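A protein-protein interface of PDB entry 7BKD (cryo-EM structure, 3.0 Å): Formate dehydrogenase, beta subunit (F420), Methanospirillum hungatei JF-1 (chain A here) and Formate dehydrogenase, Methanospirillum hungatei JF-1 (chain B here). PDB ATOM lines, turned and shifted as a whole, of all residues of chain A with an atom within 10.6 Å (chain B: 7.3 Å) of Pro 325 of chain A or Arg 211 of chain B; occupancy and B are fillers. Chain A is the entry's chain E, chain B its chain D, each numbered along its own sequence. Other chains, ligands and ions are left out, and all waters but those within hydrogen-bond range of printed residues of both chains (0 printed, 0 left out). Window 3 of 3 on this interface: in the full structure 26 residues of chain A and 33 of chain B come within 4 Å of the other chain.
Hydrophobic or aromatic side chains of chain A that line the printed part of chain B: Leu 324 and Pro 325. Along chain A the printed residues that touch a printed residue of chain B span positions 291 to 325. Of the 13 printed residues of chain B, 4 touch a printed residue of chain A. Printed residues of chain B that touch a printed residue of chain A: Glu 180, Met 208, Arg 211 and Leu 212. Hydrophobic or aromatic side chains of chain B within 4 Å of the printed part of chain A: Met 208 and Leu 212. Along chain B the printed residues that touch a printed residue of chain A span positions 180 to 212. Among the printed residues, no Asp or Glu carboxylate lies within 4 Å of a Lys or Arg side-chain nitrogen of the other chain.
The side-chain hydroxyl (OG) of Ser 291 of chain A is in hydrogen-bond range of the backbone carbonyl oxygen (O) of Ser 288 of chain A (2.7 Å). The side-chain amino group (NZ) of Lys 292 of chain A sits at hydrogen-bond distance from the backbone carbonyl oxygen (O) of Met 354 of chain A, 3.1 Å away. The side-chain carboxylate of Glu 289 of chain A is in salt-bridge range of the side-chain amino group of Lys 292 of chain A (2.9 Å). The side-chain amino group (NZ) of Lys 193 of chain B sits at hydrogen-bond distance from the backbone carbonyl oxygen (O) of Leu 212 of chain B, at 2.7 Å.
Of the printed residues of chain B, Pro 325 of chain A touches Met 208 (3.5 Å) and Arg 211 (3.7 Å). Arg 211 of chain B touches one residue of chain A. Of the printed residues of chain A, Met 208 of chain B touches Ser 291, Leu 324 and Pro 325. No residue of chain A comes within 4 Å of Ala 210 of chain B. No residue of chain A comes within 4 Å of Ala 213 of chain B. Of the printed residues of chain B, Ser 291 of chain A touches Met 208. Printed residues of chain B within 4 Å of Leu 324 of chain A: Glu 180 and Met 208. Printed residues of chain B within 4 Å of Lys 292 of chain A: Leu 212 (3.6 Å). Of the printed residues of chain A, Glu 180 of chain B touches Leu 324. Asp 214 of chain B touches none of the printed residues of chain A. Met 329 of chain A touches none of the printed residues of chain B. The nearest residue of chain B that does not touch Pro 325 of chain A is Thr 207 of chain B (5.9 Å). The nearest residue of chain A that does not touch Arg 211 of chain B is Ser 291 of chain A (5.6 Å).
The backbone carbonyl oxygen of Ser 291 of chain A sits close to the side-chain sulfur of Met 208 of chain B (3.6 Å).
Among the printed residues, pairs that only touch across the chains: Leu 324 of chain A with Glu 180 of chain B, Leu 324 of chain A with Met 208 of chain B, Pro 325 of chain A with Met 208 of chain B, Lys 292 of chain A with Leu 212 of chain B and Pro 325 of chain A with Arg 211 of chain B.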
ATOM      1  N   MET A 287     -24.939 -12.871  31.510  1.00  0.00           N
ATOM      2  CA  MET A 287     -24.975 -13.940  30.518  1.00  0.00           C
ATOM      3  C   MET A 287     -26.379 -14.508  30.362  1.00  0.00           C
ATOM      4  O   MET A 287     -26.818 -14.778  29.237  1.00  0.00           O
ATOM      5  CB  MET A 287     -23.971 -15.033  30.873  1.00  0.00           C
ATOM      6  CG  MET A 287     -22.528 -14.572  30.770  1.00  0.00           C
ATOM      7  SD  MET A 287     -21.344 -15.834  31.240  1.00  0.00           S
ATOM      8  CE  MET A 287     -21.518 -16.954  29.858  1.00  0.00           C
ATOM      9  N   SER A 288     -27.111 -14.673  31.466  1.00  0.00           N
ATOM     10  CA  SER A 288     -28.485 -15.150  31.365  1.00  0.00           C
ATOM     11  C   SER A 288     -29.357 -14.165  30.603  1.00  0.00           C
ATOM     12  O   SER A 288     -30.196 -14.569  29.791  1.00  0.00           O
ATOM     13  CB  SER A 288     -29.057 -15.403  32.758  1.00  0.00           C
ATOM     14  OG  SER A 288     -28.662 -16.673  33.247  1.00  0.00           O
ATOM     15  N   GLU A 289     -29.181 -12.867  30.854  1.00  0.00           N
ATOM     16  CA  GLU A 289     -29.948 -11.866  30.124  1.00  0.00           C
ATOM     17  C   GLU A 289     -29.614 -11.891  28.641  1.00  0.00           C
ATOM     18  O   GLU A 289     -30.511 -11.935  27.796  1.00  0.00           O
ATOM     19  CB  GLU A 289     -29.686 -10.479  30.704  1.00  0.00           C
ATOM     20  CG  GLU A 289     -30.592 -10.116  31.853  1.00  0.00           C
ATOM     21  CD  GLU A 289     -32.030 -10.492  31.589  1.00  0.00           C
ATOM     22  OE1 GLU A 289     -32.627  -9.924  30.652  1.00  0.00           O
ATOM     23  OE2 GLU A 289     -32.565 -11.354  32.316  1.00  0.00           O
ATOM     24  N   SER A 290     -28.329 -11.880  28.305  1.00  0.00           N
ATOM     25  CA  SER A 290     -27.920 -11.806  26.913  1.00  0.00           C
ATOM     26  C   SER A 290     -28.155 -13.101  26.153  1.00  0.00           C
ATOM     27  O   SER A 290     -28.076 -13.092  24.923  1.00  0.00           O
ATOM     28  CB  SER A 290     -26.448 -11.415  26.832  1.00  0.00           C
ATOM     29  OG  SER A 290     -26.222 -10.178  27.482  1.00  0.00           O
ATOM     30  N   SER A 291     -28.432 -14.209  26.840  1.00  0.00           N
ATOM     31  CA  SER A 291     -28.745 -15.437  26.121  1.00  0.00           C
ATOM     32  C   SER A 291     -30.052 -15.341  25.348  1.00  0.00           C
ATOM     33  O   SER A 291     -30.290 -16.162  24.459  1.00  0.00           O
ATOM     34  CB  SER A 291     -28.808 -16.616  27.088  1.00  0.00           C
ATOM     35  OG  SER A 291     -29.926 -16.507  27.948  1.00  0.00           O
ATOM     36  N   LYS A 292     -30.900 -14.365  25.662  1.00  0.00           N
ATOM     37  CA  LYS A 292     -32.191 -14.237  25.002  1.00  0.00           C
ATOM     38  C   LYS A 292     -32.112 -13.555  23.647  1.00  0.00           C
ATOM     39  O   LYS A 292     -33.085 -13.622  22.893  1.00  0.00           O
ATOM     40  CB  LYS A 292     -33.161 -13.454  25.883  1.00  0.00           C
ATOM     41  CG  LYS A 292     -33.402 -14.057  27.238  1.00  0.00           C
ATOM     42  CD  LYS A 292     -34.404 -13.230  28.011  1.00  0.00           C
ATOM     43  CE  LYS A 292     -33.857 -11.853  28.304  1.00  0.00           C
ATOM     44  NZ  LYS A 292     -34.813 -11.045  29.100  1.00  0.00           N
ATOM     45  N   CYS A 293     -30.994 -12.916  23.316  1.00  0.00           N
ATOM     46  CA  CYS A 293     -30.919 -12.115  22.103  1.00  0.00           C
ATOM     47  C   CYS A 293     -31.249 -12.944  20.870  1.00  0.00           C
ATOM     48  O   CYS A 293     -30.848 -14.102  20.751  1.00  0.00           O
ATOM     49  CB  CYS A 293     -29.528 -11.501  21.964  1.00  0.00           C
ATOM     50  SG  CYS A 293     -29.202 -10.767  20.358  1.00  0.00           S
ATOM     51  N   ILE A 294     -32.007 -12.342  19.955  1.00  0.00           N
ATOM     52  CA  ILE A 294     -32.391 -12.969  18.701  1.00  0.00           C
ATOM     53  C   ILE A 294     -31.747 -12.279  17.510  1.00  0.00           C
ATOM     54  O   ILE A 294     -32.148 -12.520  16.370  1.00  0.00           O
ATOM     55  CB  ILE A 294     -33.916 -13.010  18.542  1.00  0.00           C
ATOM     56  CG1 ILE A 294     -34.483 -11.595  18.523  1.00  0.00           C
ATOM     57  CG2 ILE A 294     -34.536 -13.801  19.663  1.00  0.00           C
ATOM     58  CD1 ILE A 294     -35.908 -11.519  18.070  1.00  0.00           C
ATOM     59  N   LYS A 295     -30.765 -11.415  17.751  1.00  0.00           N
ATOM     60  CA  LYS A 295     -29.972 -10.791  16.693  1.00  0.00           C
ATOM     61  C   LYS A 295     -30.829  -9.923  15.778  1.00  0.00           C
ATOM     62  O   LYS A 295     -30.677  -9.941  14.558  1.00  0.00           O
ATOM     63  CB  LYS A 295     -29.220 -11.843  15.881  1.00  0.00           C
ATOM     64  CG  LYS A 295     -28.125 -12.535  16.639  1.00  0.00           C
ATOM     65  CD  LYS A 295     -27.489 -13.605  15.788  1.00  0.00           C
ATOM     66  CE  LYS A 295     -26.676 -13.002  14.675  1.00  0.00           C
ATOM     67  NZ  LYS A 295     -25.483 -12.297  15.212  1.00  0.00           N
ATOM     68  N   TYR A 318     -16.206 -14.077  14.519  1.00  0.00           N
ATOM     69  CA  TYR A 318     -16.562 -13.695  15.877  1.00  0.00           C
ATOM     70  C   TYR A 318     -17.847 -14.368  16.337  1.00  0.00           C
ATOM     71  O   TYR A 318     -17.880 -14.977  17.409  1.00  0.00           O
ATOM     72  CB  TYR A 318     -16.715 -12.176  15.973  1.00  0.00           C
ATOM     73  CG  TYR A 318     -15.416 -11.418  15.989  1.00  0.00           C
ATOM     74  CD1 TYR A 318     -14.371 -11.813  16.804  1.00  0.00           C
ATOM     75  CD2 TYR A 318     -15.237 -10.302  15.194  1.00  0.00           C
ATOM     76  CE1 TYR A 318     -13.186 -11.121  16.822  1.00  0.00           C
ATOM     77  CE2 TYR A 318     -14.061  -9.605  15.205  1.00  0.00           C
ATOM     78  CZ  TYR A 318     -13.037 -10.016  16.022  1.00  0.00           C
ATOM     79  OH  TYR A 318     -11.854  -9.319  16.034  1.00  0.00           O
ATOM     80  N   ILE A 319     -18.907 -14.269  15.541  1.00  0.00           N
ATOM     81  CA  ILE A 319     -20.199 -14.865  15.850  1.00  0.00           C
ATOM     82  C   ILE A 319     -20.524 -15.862  14.751  1.00  0.00           C
ATOM     83  O   ILE A 319     -20.602 -15.490  13.576  1.00  0.00           O
ATOM     84  CB  ILE A 319     -21.302 -13.804  15.961  1.00  0.00           C
ATOM     85  CG1 ILE A 319     -20.961 -12.787  17.048  1.00  0.00           C
ATOM     86  CG2 ILE A 319     -22.634 -14.461  16.258  1.00  0.00           C
ATOM     87  CD1 ILE A 319     -20.835 -13.388  18.412  1.00  0.00           C
ATOM     88  N   ALA A 320     -20.724 -17.115  15.126  1.00  0.00           N
ATOM     89  CA  ALA A 320     -21.051 -18.141  14.144  1.00  0.00           C
ATOM     90  C   ALA A 320     -22.462 -17.923  13.619  1.00  0.00           C
ATOM     91  O   ALA A 320     -23.413 -17.935  14.409  1.00  0.00           O
ATOM     92  CB  ALA A 320     -20.924 -19.527  14.762  1.00  0.00           C
ATOM     93  N   PRO A 321     -22.649 -17.733  12.316  1.00  0.00           N
ATOM     94  CA  PRO A 321     -23.980 -17.393  11.805  1.00  0.00           C
ATOM     95  C   PRO A 321     -24.967 -18.534  11.979  1.00  0.00           C
ATOM     96  O   PRO A 321     -24.601 -19.711  11.985  1.00  0.00           O
ATOM     97  CB  PRO A 321     -23.732 -17.100  10.320  1.00  0.00           C
ATOM     98  CG  PRO A 321     -22.251 -17.006  10.167  1.00  0.00           C
ATOM     99  CD  PRO A 321     -21.660 -17.850  11.237  1.00  0.00           C
ATOM    100  N   GLY A 322     -26.234 -18.167  12.123  1.00  0.00           N
ATOM    101  CA  GLY A 322     -27.322 -19.123  12.209  1.00  0.00           C
ATOM    102  C   GLY A 322     -27.663 -19.622  13.596  1.00  0.00           C
ATOM    103  O   GLY A 322     -28.841 -19.753  13.931  1.00  0.00           O
ATOM    104  N   VAL A 323     -26.651 -19.915  14.409  1.00  0.00           N
ATOM    105  CA  VAL A 323     -26.884 -20.403  15.763  1.00  0.00           C
ATOM    106  C   VAL A 323     -27.560 -19.289  16.553  1.00  0.00           C
ATOM    107  O   VAL A 323     -26.956 -18.246  16.812  1.00  0.00           O
ATOM    108  CB  VAL A 323     -25.582 -20.848  16.433  1.00  0.00           C
ATOM    109  CG1 VAL A 323     -25.866 -21.416  17.811  1.00  0.00           C
ATOM    110  CG2 VAL A 323     -24.867 -21.867  15.568  1.00  0.00           C
ATOM    111  N   LEU A 324     -28.817 -19.502  16.932  1.00  0.00           N
ATOM    112  CA  LEU A 324     -29.572 -18.438  17.580  1.00  0.00           C
ATOM    113  C   LEU A 324     -29.211 -18.259  19.052  1.00  0.00           C
ATOM    114  O   LEU A 324     -29.189 -17.118  19.525  1.00  0.00           O
ATOM    115  CB  LEU A 324     -31.075 -18.657  17.437  1.00  0.00           C
ATOM    116  CG  LEU A 324     -31.805 -17.327  17.633  1.00  0.00           C
ATOM    117  CD1 LEU A 324     -31.073 -16.218  16.898  1.00  0.00           C
ATOM    118  CD2 LEU A 324     -33.248 -17.399  17.170  1.00  0.00           C
ATOM    119  N   PRO A 325     -28.932 -19.322  19.823  1.00  0.00           N
ATOM    120  CA  PRO A 325     -28.412 -19.080  21.175  1.00  0.00           C
ATOM    121  C   PRO A 325     -27.031 -18.461  21.095  1.00  0.00           C
ATOM    122  O   PRO A 325     -26.014 -19.134  21.287  1.00  0.00           O
ATOM    123  CB  PRO A 325     -28.391 -20.473  21.810  1.00  0.00           C
ATOM    124  CG  PRO A 325     -29.390 -21.243  21.045  1.00  0.00           C
ATOM    125  CD  PRO A 325     -29.315 -20.733  19.643  1.00  0.00           C
ATOM    126  N   THR A 326     -27.004 -17.168  20.791  1.00  0.00           N
ATOM    127  CA  THR A 326     -25.764 -16.473  20.493  1.00  0.00           C
ATOM    128  C   THR A 326     -24.801 -16.545  21.667  1.00  0.00           C
ATOM    129  O   THR A 326     -25.203 -16.601  22.831  1.00  0.00           O
ATOM    130  CB  THR A 326     -26.043 -15.012  20.160  1.00  0.00           C
ATOM    131  OG1 THR A 326     -26.695 -14.389  21.271  1.00  0.00           O
ATOM    132  CG2 THR A 326     -26.938 -14.917  18.967  1.00  0.00           C
ATOM    133  N   SER A 327     -23.515 -16.546  21.346  1.00  0.00           N
ATOM    134  CA  SER A 327     -22.503 -16.524  22.380  1.00  0.00           C
ATOM    135  C   SER A 327     -22.510 -15.175  23.088  1.00  0.00           C
ATOM    136  O   SER A 327     -23.061 -14.187  22.599  1.00  0.00           O
ATOM    137  CB  SER A 327     -21.124 -16.803  21.786  1.00  0.00           C
ATOM    138  OG  SER A 327     -20.133 -16.850  22.798  1.00  0.00           O
ATOM    139  N   PHE A 328     -21.879 -15.147  24.259  1.00  0.00           N
ATOM    140  CA  PHE A 328     -21.737 -13.912  25.016  1.00  0.00           C
ATOM    141  C   PHE A 328     -20.880 -12.891  24.285  1.00  0.00           C
ATOM    142  O   PHE A 328     -20.871 -11.720  24.670  1.00  0.00           O
ATOM    143  CB  PHE A 328     -21.150 -14.236  26.390  1.00  0.00           C
ATOM    144  CG  PHE A 328     -21.125 -13.076  27.337  1.00  0.00           C
ATOM    145  CD1 PHE A 328     -20.032 -12.863  28.153  1.00  0.00           C
ATOM    146  CD2 PHE A 328     -22.191 -12.209  27.422  1.00  0.00           C
ATOM    147  CE1 PHE A 328     -20.002 -11.802  29.028  1.00  0.00           C
ATOM    148  CE2 PHE A 328     -22.164 -11.145  28.296  1.00  0.00           C
ATOM    149  CZ  PHE A 328     -21.069 -10.944  29.099  1.00  0.00           C
ATOM    150  N   MET A 329     -20.172 -13.310  23.236  1.00  0.00           N
ATOM    151  CA  MET A 329     -19.294 -12.410  22.500  1.00  0.00           C
ATOM    152  C   MET A 329     -20.069 -11.281  21.834  1.00  0.00           C
ATOM    153  O   MET A 329     -19.520 -10.192  21.627  1.00  0.00           O
ATOM    154  CB  MET A 329     -18.511 -13.210  21.459  1.00  0.00           C
ATOM    155  CG  MET A 329     -17.513 -12.409  20.655  1.00  0.00           C
ATOM    156  SD  MET A 329     -16.083 -11.944  21.636  1.00  0.00           S
ATOM    157  CE  MET A 329     -15.263 -10.827  20.515  1.00  0.00           C
ATOM    158  N   PHE A 330     -21.340 -11.514  21.504  1.00  0.00           N
ATOM    159  CA  PHE A 330     -22.131 -10.514  20.794  1.00  0.00           C
ATOM    160  C   PHE A 330     -22.215  -9.220  21.584  1.00  0.00           C
ATOM    161  O   PHE A 330     -22.044  -8.129  21.033  1.00  0.00           O
ATOM    162  CB  PHE A 330     -23.531 -11.064  20.515  1.00  0.00           C
ATOM    163  CG  PHE A 330     -24.379 -10.168  19.663  1.00  0.00           C
ATOM    164  CD1 PHE A 330     -24.504 -10.397  18.311  1.00  0.00           C
ATOM    165  CD2 PHE A 330     -25.060  -9.103  20.217  1.00  0.00           C
ATOM    166  CE1 PHE A 330     -25.281  -9.579  17.533  1.00  0.00           C
ATOM    167  CE2 PHE A 330     -25.827  -8.284  19.442  1.00  0.00           C
ATOM    168  CZ  PHE A 330     -25.939  -8.521  18.100  1.00  0.00           C
ATOM    169  N   HIS A 331     -22.486  -9.320  22.882  1.00  0.00           N
ATOM    170  CA  HIS A 331     -22.589  -8.134  23.716  1.00  0.00           C
ATOM    171  C   HIS A 331     -21.241  -7.663  24.227  1.00  0.00           C
ATOM    172  O   HIS A 331     -21.100  -6.486  24.559  1.00  0.00           O
ATOM    173  CB  HIS A 331     -23.529  -8.404  24.883  1.00  0.00           C
ATOM    174  CG  HIS A 331     -24.916  -8.749  24.452  1.00  0.00           C
ATOM    175  ND1 HIS A 331     -25.263 -10.002  23.999  1.00  0.00           N
ATOM    176  CD2 HIS A 331     -26.040  -7.999  24.379  1.00  0.00           C
ATOM    177  CE1 HIS A 331     -26.542 -10.013  23.677  1.00  0.00           C
ATOM    178  NE2 HIS A 331     -27.038  -8.810  23.901  1.00  0.00           N
ATOM    179  N   MET A 354     -36.446  -8.662  23.131  1.00  0.00           N
ATOM    180  CA  MET A 354     -36.334  -9.666  24.176  1.00  0.00           C
ATOM    181  C   MET A 354     -36.200  -9.066  25.566  1.00  0.00           C
ATOM    182  O   MET A 354     -36.007  -9.810  26.530  1.00  0.00           O
ATOM    183  CB  MET A 354     -35.159 -10.589  23.877  1.00  0.00           C
ATOM    184  CG  MET A 354     -35.488 -11.669  22.870  1.00  0.00           C
ATOM    185  SD  MET A 354     -37.135 -12.356  23.112  1.00  0.00           S
ATOM    186  CE  MET A 354     -37.856 -12.138  21.492  1.00  0.00           C
ATOM    187  N   ILE A 356     -33.878  -6.966  27.109  1.00  0.00           N
ATOM    188  CA  ILE A 356     -32.552  -7.077  27.711  1.00  0.00           C
ATOM    189  C   ILE A 356     -32.118  -5.684  28.147  1.00  0.00           C
ATOM    190  O   ILE A 356     -32.154  -4.758  27.329  1.00  0.00           O
ATOM    191  CB  ILE A 356     -31.531  -7.684  26.736  1.00  0.00           C
ATOM    192  CG1 ILE A 356     -31.890  -9.130  26.418  1.00  0.00           C
ATOM    193  CG2 ILE A 356     -30.141  -7.619  27.320  1.00  0.00           C
ATOM    194  CD1 ILE A 356     -31.100  -9.698  25.286  1.00  0.00           C
ATOM    195  N   GLU B 180     -38.569 -18.234  17.838  1.00  0.00           N
ATOM    196  CA  GLU B 180     -38.076 -18.334  16.468  1.00  0.00           C
ATOM    197  C   GLU B 180     -39.036 -17.661  15.499  1.00  0.00           C
ATOM    198  O   GLU B 180     -38.677 -16.701  14.810  1.00  0.00           O
ATOM    199  CB  GLU B 180     -37.883 -19.801  16.089  1.00  0.00           C
ATOM    200  CG  GLU B 180     -36.964 -20.579  17.008  1.00  0.00           C
ATOM    201  CD  GLU B 180     -35.557 -20.030  17.023  1.00  0.00           C
ATOM    202  OE1 GLU B 180     -35.018 -19.816  18.127  1.00  0.00           O
ATOM    203  OE2 GLU B 180     -34.991 -19.814  15.932  1.00  0.00           O
ATOM    204  N   LYS B 193     -41.520 -13.999  32.451  1.00  0.00           N
ATOM    205  CA  LYS B 193     -40.386 -14.530  33.197  1.00  0.00           C
ATOM    206  C   LYS B 193     -39.817 -13.480  34.137  1.00  0.00           C
ATOM    207  O   LYS B 193     -39.476 -13.781  35.285  1.00  0.00           O
ATOM    208  CB  LYS B 193     -39.308 -15.019  32.233  1.00  0.00           C
ATOM    209  CG  LYS B 193     -38.051 -15.506  32.912  1.00  0.00           C
ATOM    210  CD  LYS B 193     -36.953 -15.757  31.907  1.00  0.00           C
ATOM    211  CE  LYS B 193     -36.010 -16.827  32.409  1.00  0.00           C
ATOM    212  NZ  LYS B 193     -36.772 -17.972  32.975  1.00  0.00           N
ATOM    213  N   ALA B 201     -42.244 -25.584  29.160  1.00  0.00           N
ATOM    214  CA  ALA B 201     -42.105 -25.828  27.732  1.00  0.00           C
ATOM    215  C   ALA B 201     -42.161 -27.323  27.471  1.00  0.00           C
ATOM    216  O   ALA B 201     -41.546 -28.106  28.199  1.00  0.00           O
ATOM    217  CB  ALA B 201     -40.797 -25.249  27.199  1.00  0.00           C
ATOM    218  N   TYR B 206     -34.993 -28.919  22.361  1.00  0.00           N
ATOM    219  CA  TYR B 206     -34.640 -27.825  23.266  1.00  0.00           C
ATOM    220  C   TYR B 206     -34.258 -26.608  22.433  1.00  0.00           C
ATOM    221  O   TYR B 206     -33.181 -26.564  21.835  1.00  0.00           O
ATOM    222  CB  TYR B 206     -33.505 -28.259  24.185  1.00  0.00           C
ATOM    223  CG  TYR B 206     -33.189 -27.309  25.315  1.00  0.00           C
ATOM    224  CD1 TYR B 206     -33.904 -27.347  26.499  1.00  0.00           C
ATOM    225  CD2 TYR B 206     -32.157 -26.392  25.204  1.00  0.00           C
ATOM    226  CE1 TYR B 206     -33.611 -26.488  27.537  1.00  0.00           C
ATOM    227  CE2 TYR B 206     -31.856 -25.532  26.235  1.00  0.00           C
ATOM    228  CZ  TYR B 206     -32.586 -25.582  27.399  1.00  0.00           C
ATOM    229  OH  TYR B 206     -32.285 -24.722  28.427  1.00  0.00           O
ATOM    230  N   THR B 207     -35.139 -25.611  22.393  1.00  0.00           N
ATOM    231  CA  THR B 207     -34.979 -24.439  21.545  1.00  0.00           C
ATOM    232  C   THR B 207     -34.804 -23.172  22.373  1.00  0.00           C
ATOM    233  O   THR B 207     -34.687 -23.211  23.601  1.00  0.00           O
ATOM    234  CB  THR B 207     -36.171 -24.290  20.604  1.00  0.00           C
ATOM    235  OG1 THR B 207     -37.387 -24.465  21.340  1.00  0.00           O
ATOM    236  CG2 THR B 207     -36.096 -25.286  19.480  1.00  0.00           C
ATOM    237  N   MET B 208     -34.784 -22.036  21.674  1.00  0.00           N
ATOM    238  CA  MET B 208     -34.709 -20.740  22.338  1.00  0.00           C
ATOM    239  C   MET B 208     -35.901 -20.519  23.256  1.00  0.00           C
ATOM    240  O   MET B 208     -35.753 -19.983  24.359  1.00  0.00           O
ATOM    241  CB  MET B 208     -34.640 -19.630  21.294  1.00  0.00           C
ATOM    242  CG  MET B 208     -34.444 -18.244  21.872  1.00  0.00           C
ATOM    243  SD  MET B 208     -32.883 -18.028  22.729  1.00  0.00           S
ATOM    244  CE  MET B 208     -31.786 -17.997  21.327  1.00  0.00           C
ATOM    245  N   THR B 209     -37.097 -20.904  22.810  1.00  0.00           N
ATOM    246  CA  THR B 209     -38.286 -20.705  23.630  1.00  0.00           C
ATOM    247  C   THR B 209     -38.224 -21.541  24.900  1.00  0.00           C
ATOM    248  O   THR B 209     -38.618 -21.080  25.976  1.00  0.00           O
ATOM    249  CB  THR B 209     -39.539 -21.045  22.826  1.00  0.00           C
ATOM    250  OG1 THR B 209     -39.610 -20.193  21.677  1.00  0.00           O
ATOM    251  CG2 THR B 209     -40.779 -20.837  23.667  1.00  0.00           C
ATOM    252  N   ALA B 210     -37.730 -22.773  24.797  1.00  0.00           N
ATOM    253  CA  ALA B 210     -37.624 -23.629  25.967  1.00  0.00           C
ATOM    254  C   ALA B 210     -36.533 -23.182  26.927  1.00  0.00           C
ATOM    255  O   ALA B 210     -36.481 -23.686  28.052  1.00  0.00           O
ATOM    256  CB  ALA B 210     -37.376 -25.074  25.541  1.00  0.00           C
ATOM    257  N   ARG B 211     -35.660 -22.264  26.515  1.00  0.00           N
ATOM    258  CA  ARG B 211     -34.641 -21.758  27.425  1.00  0.00           C
ATOM    259  C   ARG B 211     -35.207 -20.756  28.417  1.00  0.00           C
ATOM    260  O   ARG B 211     -34.697 -20.646  29.537  1.00  0.00           O
ATOM    261  CB  ARG B 211     -33.494 -21.132  26.637  1.00  0.00           C
ATOM    262  CG  ARG B 211     -32.620 -22.154  25.945  1.00  0.00           C
ATOM    263  CD  ARG B 211     -31.816 -21.542  24.817  1.00  0.00           C
ATOM    264  NE  ARG B 211     -30.886 -22.498  24.225  1.00  0.00           N
ATOM    265  CZ  ARG B 211     -29.824 -23.003  24.845  1.00  0.00           C
ATOM    266  NH1 ARG B 211     -29.531 -22.640  26.085  1.00  0.00           N
ATOM    267  NH2 ARG B 211     -29.043 -23.869  24.216  1.00  0.00           N
ATOM    268  N   LEU B 212     -36.248 -20.017  28.032  1.00  0.00           N
ATOM    269  CA  LEU B 212     -36.915 -19.126  28.971  1.00  0.00           C
ATOM    270  C   LEU B 212     -37.691 -19.888  30.031  1.00  0.00           C
ATOM    271  O   LEU B 212     -38.056 -19.303  31.054  1.00  0.00           O
ATOM    272  CB  LEU B 212     -37.868 -18.193  28.230  1.00  0.00           C
ATOM    273  CG  LEU B 212     -37.272 -17.294  27.152  1.00  0.00           C
ATOM    274  CD1 LEU B 212     -38.338 -16.907  26.147  1.00  0.00           C
ATOM    275  CD2 LEU B 212     -36.657 -16.062  27.781  1.00  0.00           C
ATOM    276  N   ALA B 213     -37.944 -21.171  29.811  1.00  0.00           N
ATOM    277  CA  ALA B 213     -38.838 -21.923  30.674  1.00  0.00           C
ATOM    278  C   ALA B 213     -38.197 -22.207  32.025  1.00  0.00           C
ATOM    279  O   ALA B 213     -36.979 -22.348  32.146  1.00  0.00           O
ATOM    280  CB  ALA B 213     -39.236 -23.235  30.007  1.00  0.00           C
ATOM    281  N   ASP B 214     -39.043 -22.281  33.052  1.00  0.00           N
ATOM    282  CA  ASP B 214     -38.582 -22.752  34.351  1.00  0.00           C
ATOM    283  C   ASP B 214     -38.383 -24.260  34.338  1.00  0.00           C
ATOM    284  O   ASP B 214     -37.424 -24.772  34.924  1.00  0.00           O
ATOM    285  CB  ASP B 214     -39.577 -22.353  35.439  1.00  0.00           C
ATOM    286  CG  ASP B 214     -39.839 -20.859  35.470  1.00  0.00           C
ATOM    287  OD1 ASP B 214     -38.994 -20.091  34.967  1.00  0.00           O
ATOM    288  OD2 ASP B 214     -40.890 -20.452  36.006  1.00  0.00           O
ATOM    289  N   TYR B 216     -38.468 -27.783  31.644  1.00  0.00           N
ATOM    290  CA  TYR B 216     -38.439 -28.246  30.266  1.00  0.00           C
ATOM    291  C   TYR B 216     -38.780 -29.725  30.235  1.00  0.00           C
ATOM    292  O   TYR B 216     -38.214 -30.511  31.000  1.00  0.00           O
ATOM    293  CB  TYR B 216     -37.074 -28.010  29.626  1.00  0.00           C
ATOM    294  CG  TYR B 216     -36.904 -28.718  28.307  1.00  0.00           C
ATOM    295  CD1 TYR B 216     -37.769 -28.479  27.255  1.00  0.00           C
ATOM    296  CD2 TYR B 216     -35.878 -29.629  28.116  1.00  0.00           C
ATOM    297  CE1 TYR B 216     -37.617 -29.123  26.052  1.00  0.00           C
ATOM    298  CE2 TYR B 216     -35.719 -30.277  26.914  1.00  0.00           C
ATOM    299  CZ  TYR B 216     -36.591 -30.021  25.886  1.00  0.00           C
ATOM    300  OH  TYR B 216     -36.435 -30.668  24.684  1.00  0.00           O
